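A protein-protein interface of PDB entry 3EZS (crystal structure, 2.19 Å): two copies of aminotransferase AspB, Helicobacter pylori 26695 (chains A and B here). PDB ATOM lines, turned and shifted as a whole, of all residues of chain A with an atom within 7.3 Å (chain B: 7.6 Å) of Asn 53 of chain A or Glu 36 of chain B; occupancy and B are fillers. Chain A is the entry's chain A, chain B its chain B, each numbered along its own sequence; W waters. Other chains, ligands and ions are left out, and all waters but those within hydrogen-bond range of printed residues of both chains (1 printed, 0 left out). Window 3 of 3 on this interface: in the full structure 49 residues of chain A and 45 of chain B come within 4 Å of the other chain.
O of Leu 52 of chain A lies close to N of Pro 236 of chain B, at 3.4 Å.
The backbone NH of Gly 237 of chain B is in hydrogen-bond range of the backbone carbonyl oxygen of Leu 52 of chain A (2.8 Å).
The side-chain hydroxyl (OG1) of Thr 49 of chain A lies within hydrogen-bond range of the side-chain amide oxygen (OE1) of Gln 42 of chain B.
The backbone NH (N) of Asn 53 of chain A sits at hydrogen-bond distance from the side-chain hydroxyl (OG1) of Thr 37 of chain B (3.0 Å).
The side-chain amide oxygen of Gln 42 of chain B sits at hydrogen-bond distance from the backbone NH of His 50 of chain A, 3.2 Å away.
The side-chain amide nitrogen (ND2) of Asn 53 of chain A sits at hydrogen-bond distance from the backbone carbonyl oxygen (O) of Phe 35 of chain B (3.0 Å).
NE2 of Gln 42 of chain B lies within hydrogen-bond range of O of Thr 37 of chain B, 2.9 Å away.
The side-chain hydroxyl of Thr 37 of chain B lies within hydrogen-bond range of the backbone carbonyl oxygen of Ser 234 of chain B (2.8 Å).
O of Ser 230 of chain B is in hydrogen-bond range of N of Ala 235 of chain B (3.1 Å).
OD1 of Asn 53 of chain A lies close to O of His 50 of chain A (3.1 Å).
Thr 37 of chain B touches Leu 52 of chain A (OG1 to C, 3.2 Å).
CA of Ala 235 of chain B touches O of Leu 52 of chain A, at 3.5 Å.
Leu 238 of chain B touches Leu 52 of chain A (CD2 to CD2, 3.8 Å).
Glu 36 of chain B touches Asn 53 of chain A (OE1 to ND2, 3.8 Å).
CA of Asn 53 of chain A touches O of Ser 234 of chain B, 3.7 Å away.
Asn 53 of chain A touches Pro 236 of chain B.
C of Ile 54 of chain A touches CG of Pro 236 of chain B (3.8 Å).
Gly 237 of chain B touches Ile 54 of chain A.
Tyr 55 of chain A touches Pro 236 of chain B.
Ser 51 of chain A touches none of the printed residues of chain B.
Printed residues of chain B within 4 Å of Asn 53 of chain A: Phe 35, Glu 36, Thr 37, Ser 234 and Pro 236.
Of the printed residues of chain A, Phe 35 of chain B touches Asn 53.
Glu 36 of chain B touches one residue of chain A.
Of the printed residues of chain A, Thr 37 of chain B touches Leu 52 (3.2 Å) and Asn 53 (3.0 Å).
The nearest residue of chain A that does not touch Glu 36 of chain B is His 50 of chain A (4.4 Å).
The nearest printed residue of chain A that does not touch Thr 37 of chain B is His 50 of chain A (4.9 Å).
Hydrophobic or aromatic side chains of chain A within 4 Å of the printed part of chain B: Leu 52 and Tyr 55.
Of the 19 printed residues of chain B, 9 touch a printed residue of chain A.
Hydrophobic or aromatic side chains of chain B within 4 Å of the printed part of chain A: Pro 236 and Leu 238.
Among the printed residues, 15 pairs touch across the chains.
Among the printed residues, no Asp or Glu carboxylate lies within 4 Å of a Lys or Arg side-chain nitrogen of the other chain.
No position is printed for both chains.
Water W1 lies within hydrogen-bond range of the backbone carbonyl oxygen (O) of His 50 of chain A (2.6 Å), the side-chain carboxylate (OE1) of Glu 36 of chain B (2.8 Å) and the backbone NH (N) of Thr 37 of chain B (2.9 Å).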
ATOM      1  N   THR A  49      -5.612  -8.775  -3.003  1.00  0.00           N
ATOM      2  CA  THR A  49      -5.668  -7.550  -2.186  1.00  0.00           C
ATOM      3  C   THR A  49      -4.358  -7.218  -1.475  1.00  0.00           C
ATOM      4  O   THR A  49      -4.101  -6.054  -1.168  1.00  0.00           O
ATOM      5  CB  THR A  49      -6.811  -7.601  -1.153  1.00  0.00           C
ATOM      6  OG1 THR A  49      -6.600  -8.703  -0.261  1.00  0.00           O
ATOM      7  CG2 THR A  49      -8.176  -7.743  -1.865  1.00  0.00           C
ATOM      8  N   HIS A  50      -3.545  -8.239  -1.212  1.00  0.00           N
ATOM      9  CA  HIS A  50      -2.228  -8.078  -0.599  1.00  0.00           C
ATOM     10  C   HIS A  50      -1.310  -7.113  -1.363  1.00  0.00           C
ATOM     11  O   HIS A  50      -0.433  -6.504  -0.765  1.00  0.00           O
ATOM     12  CB  HIS A  50      -1.524  -9.446  -0.467  1.00  0.00           C
ATOM     13  CG  HIS A  50      -1.307 -10.146  -1.777  1.00  0.00           C
ATOM     14  ND1 HIS A  50      -0.131 -10.044  -2.493  1.00  0.00           N
ATOM     15  CD2 HIS A  50      -2.118 -10.954  -2.502  1.00  0.00           C
ATOM     16  CE1 HIS A  50      -0.235 -10.746  -3.607  1.00  0.00           C
ATOM     17  NE2 HIS A  50      -1.430 -11.307  -3.638  1.00  0.00           N
ATOM     18  N   SER A  51      -1.514  -6.952  -2.667  1.00  0.00           N
ATOM     19  CA  SER A  51      -0.661  -6.041  -3.469  1.00  0.00           C
ATOM     20  C   SER A  51      -0.978  -4.525  -3.319  1.00  0.00           C
ATOM     21  O   SER A  51      -0.420  -3.700  -4.062  1.00  0.00           O
ATOM     22  CB  SER A  51      -0.735  -6.424  -4.948  1.00  0.00           C
ATOM     23  OG  SER A  51      -2.031  -6.197  -5.478  1.00  0.00           O
ATOM     24  N   LEU A  52      -1.876  -4.176  -2.391  1.00  0.00           N
ATOM     25  CA  LEU A  52      -2.258  -2.780  -2.129  1.00  0.00           C
ATOM     26  C   LEU A  52      -1.107  -1.932  -1.605  1.00  0.00           C
ATOM     27  O   LEU A  52      -1.141  -0.702  -1.717  1.00  0.00           O
ATOM     28  CB  LEU A  52      -3.437  -2.702  -1.145  1.00  0.00           C
ATOM     29  CG  LEU A  52      -4.843  -2.958  -1.712  1.00  0.00           C
ATOM     30  CD1 LEU A  52      -5.912  -2.923  -0.597  1.00  0.00           C
ATOM     31  CD2 LEU A  52      -5.179  -1.965  -2.818  1.00  0.00           C
ATOM     32  N   ASN A  53      -0.094  -2.584  -1.053  1.00  0.00           N
ATOM     33  CA  ASN A  53       1.087  -1.892  -0.549  1.00  0.00           C
ATOM     34  C   ASN A  53       2.131  -1.565  -1.617  1.00  0.00           C
ATOM     35  O   ASN A  53       3.145  -0.975  -1.306  1.00  0.00           O
ATOM     36  CB  ASN A  53       1.740  -2.664   0.605  1.00  0.00           C
ATOM     37  CG  ASN A  53       2.363  -4.004   0.179  1.00  0.00           C
ATOM     38  OD1 ASN A  53       1.971  -4.620  -0.806  1.00  0.00           O
ATOM     39  ND2 ASN A  53       3.335  -4.456   0.953  1.00  0.00           N
ATOM     40  N   ILE A  54       1.875  -1.931  -2.869  1.00  0.00           N
ATOM     41  CA  ILE A  54       2.810  -1.691  -3.970  1.00  0.00           C
ATOM     42  C   ILE A  54       2.350  -0.468  -4.776  1.00  0.00           C
ATOM     43  O   ILE A  54       1.183  -0.372  -5.158  1.00  0.00           O
ATOM     44  CB  ILE A  54       2.890  -2.929  -4.907  1.00  0.00           C
ATOM     45  CG1 ILE A  54       3.242  -4.208  -4.128  1.00  0.00           C
ATOM     46  CG2 ILE A  54       3.882  -2.703  -6.056  1.00  0.00           C
ATOM     47  CD1 ILE A  54       4.536  -4.147  -3.326  1.00  0.00           C
ATOM     48  N   TYR A  55       3.269   0.461  -5.022  1.00  0.00           N
ATOM     49  CA  TYR A  55       2.956   1.658  -5.790  1.00  0.00           C
ATOM     50  C   TYR A  55       2.825   1.215  -7.254  1.00  0.00           C
ATOM     51  O   TYR A  55       3.792   0.746  -7.848  1.00  0.00           O
ATOM     52  CB  TYR A  55       4.057   2.717  -5.613  1.00  0.00           C
ATOM     53  CG  TYR A  55       3.613   4.129  -5.960  1.00  0.00           C
ATOM     54  CD1 TYR A  55       3.437   4.527  -7.298  1.00  0.00           C
ATOM     55  CD2 TYR A  55       3.387   5.070  -4.961  1.00  0.00           C
ATOM     56  CE1 TYR A  55       3.027   5.829  -7.630  1.00  0.00           C
ATOM     57  CE2 TYR A  55       2.982   6.375  -5.276  1.00  0.00           C
ATOM     58  CZ  TYR A  55       2.803   6.755  -6.617  1.00  0.00           C
ATOM     59  OH  TYR A  55       2.414   8.054  -6.936  1.00  0.00           O
ATOM     60  N   PRO A  56       1.634   1.340  -7.840  1.00  0.00           N
ATOM     61  CA  PRO A  56       1.517   0.835  -9.226  1.00  0.00           C
ATOM     62  C   PRO A  56       2.296   1.627 -10.290  1.00  0.00           C
ATOM     63  O   PRO A  56       2.472   2.835 -10.157  1.00  0.00           O
ATOM     64  CB  PRO A  56       0.018   0.907  -9.522  1.00  0.00           C
ATOM     65  CG  PRO A  56      -0.657   1.421  -8.276  1.00  0.00           C
ATOM     66  CD  PRO A  56       0.382   1.925  -7.334  1.00  0.00           C
ATOM     67  N   GLU B  32       8.901   4.864  -0.747  1.00  0.00           N
ATOM     68  CA  GLU B  32       7.607   4.207  -0.526  1.00  0.00           C
ATOM     69  C   GLU B  32       7.665   3.238   0.669  1.00  0.00           C
ATOM     70  O   GLU B  32       8.652   2.505   0.811  1.00  0.00           O
ATOM     71  CB  GLU B  32       7.211   3.419  -1.777  1.00  0.00           C
ATOM     72  N   PRO B  33       6.613   3.228   1.532  1.00  0.00           N
ATOM     73  CA  PRO B  33       6.542   2.291   2.659  1.00  0.00           C
ATOM     74  C   PRO B  33       6.669   0.838   2.212  1.00  0.00           C
ATOM     75  O   PRO B  33       6.129   0.479   1.173  1.00  0.00           O
ATOM     76  CB  PRO B  33       5.134   2.514   3.221  1.00  0.00           C
ATOM     77  CG  PRO B  33       4.728   3.833   2.777  1.00  0.00           C
ATOM     78  CD  PRO B  33       5.441   4.125   1.500  1.00  0.00           C
ATOM     79  N   GLN B  34       7.380   0.034   2.997  1.00  0.00           N
ATOM     80  CA  GLN B  34       7.599  -1.383   2.734  1.00  0.00           C
ATOM     81  C   GLN B  34       6.875  -2.184   3.796  1.00  0.00           C
ATOM     82  O   GLN B  34       7.457  -3.079   4.406  1.00  0.00           O
ATOM     83  CB  GLN B  34       9.095  -1.707   2.795  1.00  0.00           C
ATOM     84  CG  GLN B  34       9.945  -0.843   1.892  1.00  0.00           C
ATOM     85  CD  GLN B  34       9.601  -1.001   0.431  1.00  0.00           C
ATOM     86  OE1 GLN B  34       9.680  -2.096  -0.124  1.00  0.00           O
ATOM     87  NE2 GLN B  34       9.230   0.103  -0.206  1.00  0.00           N
ATOM     88  N   PHE B  35       5.621  -1.833   4.057  1.00  0.00           N
ATOM     89  CA  PHE B  35       4.825  -2.531   5.053  1.00  0.00           C
ATOM     90  C   PHE B  35       3.594  -3.091   4.365  1.00  0.00           C
ATOM     91  O   PHE B  35       3.177  -2.601   3.315  1.00  0.00           O
ATOM     92  CB  PHE B  35       4.381  -1.603   6.187  1.00  0.00           C
ATOM     93  CG  PHE B  35       5.501  -0.862   6.853  1.00  0.00           C
ATOM     94  CD1 PHE B  35       6.538  -1.551   7.473  1.00  0.00           C
ATOM     95  CD2 PHE B  35       5.497   0.521   6.910  1.00  0.00           C
ATOM     96  CE1 PHE B  35       7.563  -0.870   8.107  1.00  0.00           C
ATOM     97  CE2 PHE B  35       6.532   1.206   7.546  1.00  0.00           C
ATOM     98  CZ  PHE B  35       7.561   0.510   8.143  1.00  0.00           C
ATOM     99  N   GLU B  36       3.011  -4.107   4.978  1.00  0.00           N
ATOM    100  CA  GLU B  36       1.818  -4.732   4.461  1.00  0.00           C
ATOM    101  C   GLU B  36       0.658  -3.779   4.660  1.00  0.00           C
ATOM    102  O   GLU B  36       0.666  -2.983   5.594  1.00  0.00           O
ATOM    103  CB  GLU B  36       1.535  -6.035   5.201  1.00  0.00           C
ATOM    104  CG  GLU B  36       2.640  -7.107   5.115  1.00  0.00           C
ATOM    105  CD  GLU B  36       2.782  -7.783   3.752  1.00  0.00           C
ATOM    106  OE1 GLU B  36       1.998  -7.486   2.818  1.00  0.00           O
ATOM    107  OE2 GLU B  36       3.686  -8.649   3.629  1.00  0.00           O
ATOM    108  N   THR B  37      -0.321  -3.829   3.761  1.00  0.00           N
ATOM    109  CA  THR B  37      -1.511  -3.005   3.908  1.00  0.00           C
ATOM    110  C   THR B  37      -2.336  -3.656   5.007  1.00  0.00           C
ATOM    111  O   THR B  37      -2.497  -4.877   4.988  1.00  0.00           O
ATOM    112  CB  THR B  37      -2.326  -2.935   2.612  1.00  0.00           C
ATOM    113  OG1 THR B  37      -1.531  -2.315   1.594  1.00  0.00           O
ATOM    114  CG2 THR B  37      -3.622  -2.126   2.838  1.00  0.00           C
ATOM    115  N   PRO B  38      -2.800  -2.871   6.002  1.00  0.00           N
ATOM    116  CA  PRO B  38      -3.628  -3.442   7.066  1.00  0.00           C
ATOM    117  C   PRO B  38      -4.755  -4.357   6.579  1.00  0.00           C
ATOM    118  O   PRO B  38      -5.396  -4.081   5.579  1.00  0.00           O
ATOM    119  CB  PRO B  38      -4.189  -2.202   7.759  1.00  0.00           C
ATOM    120  CG  PRO B  38      -3.106  -1.196   7.614  1.00  0.00           C
ATOM    121  CD  PRO B  38      -2.540  -1.435   6.244  1.00  0.00           C
ATOM    122  N   LYS B  39      -4.965  -5.444   7.302  1.00  0.00           N
ATOM    123  CA  LYS B  39      -5.958  -6.464   6.957  1.00  0.00           C
ATOM    124  C   LYS B  39      -7.379  -5.901   6.812  1.00  0.00           C
ATOM    125  O   LYS B  39      -8.107  -6.283   5.894  1.00  0.00           O
ATOM    126  CB  LYS B  39      -5.948  -7.584   8.017  1.00  0.00           C
ATOM    127  CG  LYS B  39      -6.575  -8.921   7.546  1.00  0.00           C
ATOM    128  CD  LYS B  39      -5.613  -9.686   6.585  1.00  0.00           C
ATOM    129  CE  LYS B  39      -6.319 -10.682   5.641  1.00  0.00           C
ATOM    130  NZ  LYS B  39      -7.028 -10.007   4.499  1.00  0.00           N
ATOM    131  N   ILE B  41      -8.324  -3.038   5.783  1.00  0.00           N
ATOM    132  CA  ILE B  41      -8.407  -2.290   4.518  1.00  0.00           C
ATOM    133  C   ILE B  41      -8.560  -3.303   3.383  1.00  0.00           C
ATOM    134  O   ILE B  41      -9.389  -3.123   2.495  1.00  0.00           O
ATOM    135  CB  ILE B  41      -7.153  -1.380   4.298  1.00  0.00           C
ATOM    136  CG1 ILE B  41      -7.074  -0.299   5.373  1.00  0.00           C
ATOM    137  CG2 ILE B  41      -7.169  -0.727   2.925  1.00  0.00           C
ATOM    138  CD1 ILE B  41      -5.723   0.348   5.497  1.00  0.00           C
ATOM    139  N   GLN B  42      -7.793  -4.394   3.442  1.00  0.00           N
ATOM    140  CA  GLN B  42      -7.906  -5.448   2.448  1.00  0.00           C
ATOM    141  C   GLN B  42      -9.293  -6.138   2.490  1.00  0.00           C
ATOM    142  O   GLN B  42      -9.873  -6.459   1.459  1.00  0.00           O
ATOM    143  CB  GLN B  42      -6.798  -6.468   2.644  1.00  0.00           C
ATOM    144  CG  GLN B  42      -5.383  -5.944   2.373  1.00  0.00           C
ATOM    145  CD  GLN B  42      -4.372  -7.070   2.375  1.00  0.00           C
ATOM    146  OE1 GLN B  42      -4.613  -8.138   1.797  1.00  0.00           O
ATOM    147  NE2 GLN B  42      -3.244  -6.854   3.042  1.00  0.00           N
ATOM    148  N   SER B 230      -1.471   7.294   0.835  1.00  0.00           N
ATOM    149  CA  SER B 230      -0.413   6.316   0.536  1.00  0.00           C
ATOM    150  C   SER B 230       0.571   5.952   1.642  1.00  0.00           C
ATOM    151  O   SER B 230       0.755   4.755   1.962  1.00  0.00           O
ATOM    152  CB  SER B 230       0.374   6.751  -0.706  1.00  0.00           C
ATOM    153  OG  SER B 230      -0.472   6.776  -1.840  1.00  0.00           O
ATOM    154  N   SER B 233      -1.153   5.083   5.405  1.00  0.00           N
ATOM    155  CA  SER B 233      -1.734   3.741   5.603  1.00  0.00           C
ATOM    156  C   SER B 233      -1.029   2.565   4.912  1.00  0.00           C
ATOM    157  O   SER B 233      -1.512   1.421   4.989  1.00  0.00           O
ATOM    158  CB  SER B 233      -3.176   3.811   5.132  1.00  0.00           C
ATOM    159  OG  SER B 233      -3.798   4.909   5.771  1.00  0.00           O
ATOM    160  N   SER B 234       0.139   2.837   4.309  1.00  0.00           N
ATOM    161  CA  SER B 234       0.887   1.812   3.583  1.00  0.00           C
ATOM    162  C   SER B 234      -0.031   1.194   2.520  1.00  0.00           C
ATOM    163  O   SER B 234      -0.103  -0.030   2.388  1.00  0.00           O
ATOM    164  CB  SER B 234       1.411   0.713   4.527  1.00  0.00           C
ATOM    165  OG  SER B 234       2.198   1.231   5.580  1.00  0.00           O
ATOM    166  N   ALA B 235      -0.740   2.051   1.779  1.00  0.00           N
ATOM    167  CA  ALA B 235      -1.709   1.617   0.774  1.00  0.00           C
ATOM    168  C   ALA B 235      -1.669   2.477  -0.476  1.00  0.00           C
ATOM    169  O   ALA B 235      -2.708   3.004  -0.902  1.00  0.00           O
ATOM    170  CB  ALA B 235      -3.144   1.645   1.393  1.00  0.00           C
ATOM    171  N   PRO B 236      -0.484   2.587  -1.113  1.00  0.00           N
ATOM    172  CA  PRO B 236      -0.419   3.389  -2.334  1.00  0.00           C
ATOM    173  C   PRO B 236      -1.310   2.831  -3.440  1.00  0.00           C
ATOM    174  O   PRO B 236      -1.772   3.581  -4.274  1.00  0.00           O
ATOM    175  CB  PRO B 236       1.066   3.316  -2.735  1.00  0.00           C
ATOM    176  CG  PRO B 236       1.568   2.061  -2.103  1.00  0.00           C
ATOM    177  CD  PRO B 236       0.817   1.961  -0.805  1.00  0.00           C
ATOM    178  N   GLY B 237      -1.567   1.525  -3.430  1.00  0.00           N
ATOM    179  CA  GLY B 237      -2.414   0.900  -4.446  1.00  0.00           C
ATOM    180  C   GLY B 237      -3.860   1.351  -4.434  1.00  0.00           C
ATOM    181  O   GLY B 237      -4.561   1.161  -5.416  1.00  0.00           O
ATOM    182  N   LEU B 238      -4.319   1.925  -3.320  1.00  0.00           N
ATOM    183  CA  LEU B 238      -5.678   2.441  -3.238  1.00  0.00           C
ATOM    184  C   LEU B 238      -5.882   3.673  -4.120  1.00  0.00           C
ATOM    185  O   LEU B 238      -6.987   3.890  -4.603  1.00  0.00           O
ATOM    186  CB  LEU B 238      -6.087   2.741  -1.786  1.00  0.00           C
ATOM    187  CG  LEU B 238      -6.415   1.552  -0.875  1.00  0.00           C
ATOM    188  CD1 LEU B 238      -6.793   1.992   0.549  1.00  0.00           C
ATOM    189  CD2 LEU B 238      -7.545   0.729  -1.479  1.00  0.00           C
ATOM    190  N   PHE B 284       0.241   3.213  14.292  1.00  0.00           N
ATOM    191  CA  PHE B 284       1.146   2.062  14.311  1.00  0.00           C
ATOM    192  C   PHE B 284       2.332   2.315  13.360  1.00  0.00           C
ATOM    193  O   PHE B 284       3.484   2.164  13.753  1.00  0.00           O
ATOM    194  CB  PHE B 284       0.386   0.805  13.883  1.00  0.00           C
ATOM    195  CG  PHE B 284       1.231  -0.444  13.789  1.00  0.00           C
ATOM    196  CD1 PHE B 284       1.427  -1.249  14.901  1.00  0.00           C
ATOM    197  CD2 PHE B 284       1.790  -0.840  12.572  1.00  0.00           C
ATOM    198  CE1 PHE B 284       2.189  -2.414  14.815  1.00  0.00           C
ATOM    199  CE2 PHE B 284       2.547  -2.010  12.478  1.00  0.00           C
ATOM    200  CZ  PHE B 284       2.741  -2.793  13.594  1.00  0.00           C
ATOM    201  N   PHE B 285       2.047   2.735  12.131  1.00  0.00           N
ATOM    202  CA  PHE B 285       3.111   2.977  11.167  1.00  0.00           C
ATOM    203  C   PHE B 285       3.934   4.204  11.546  1.00  0.00           C
ATOM    204  O   PHE B 285       5.166   4.205  11.389  1.00  0.00           O
ATOM    205  CB  PHE B 285       2.589   3.118   9.726  1.00  0.00           C
ATOM    206  CG  PHE B 285       1.950   1.856   9.162  1.00  0.00           C
ATOM    207  CD1 PHE B 285       2.604   0.646   9.209  1.00  0.00           C
ATOM    208  CD2 PHE B 285       0.717   1.909   8.515  1.00  0.00           C
ATOM    209  CE1 PHE B 285       2.023  -0.511   8.686  1.00  0.00           C
ATOM    210  CE2 PHE B 285       0.134   0.750   7.971  1.00  0.00           C
ATOM    211  CZ  PHE B 285       0.790  -0.453   8.067  1.00  0.00           C
HETATM  212  O   HOH W   1      -0.068  -5.909   1.739  1.00  0.00           O
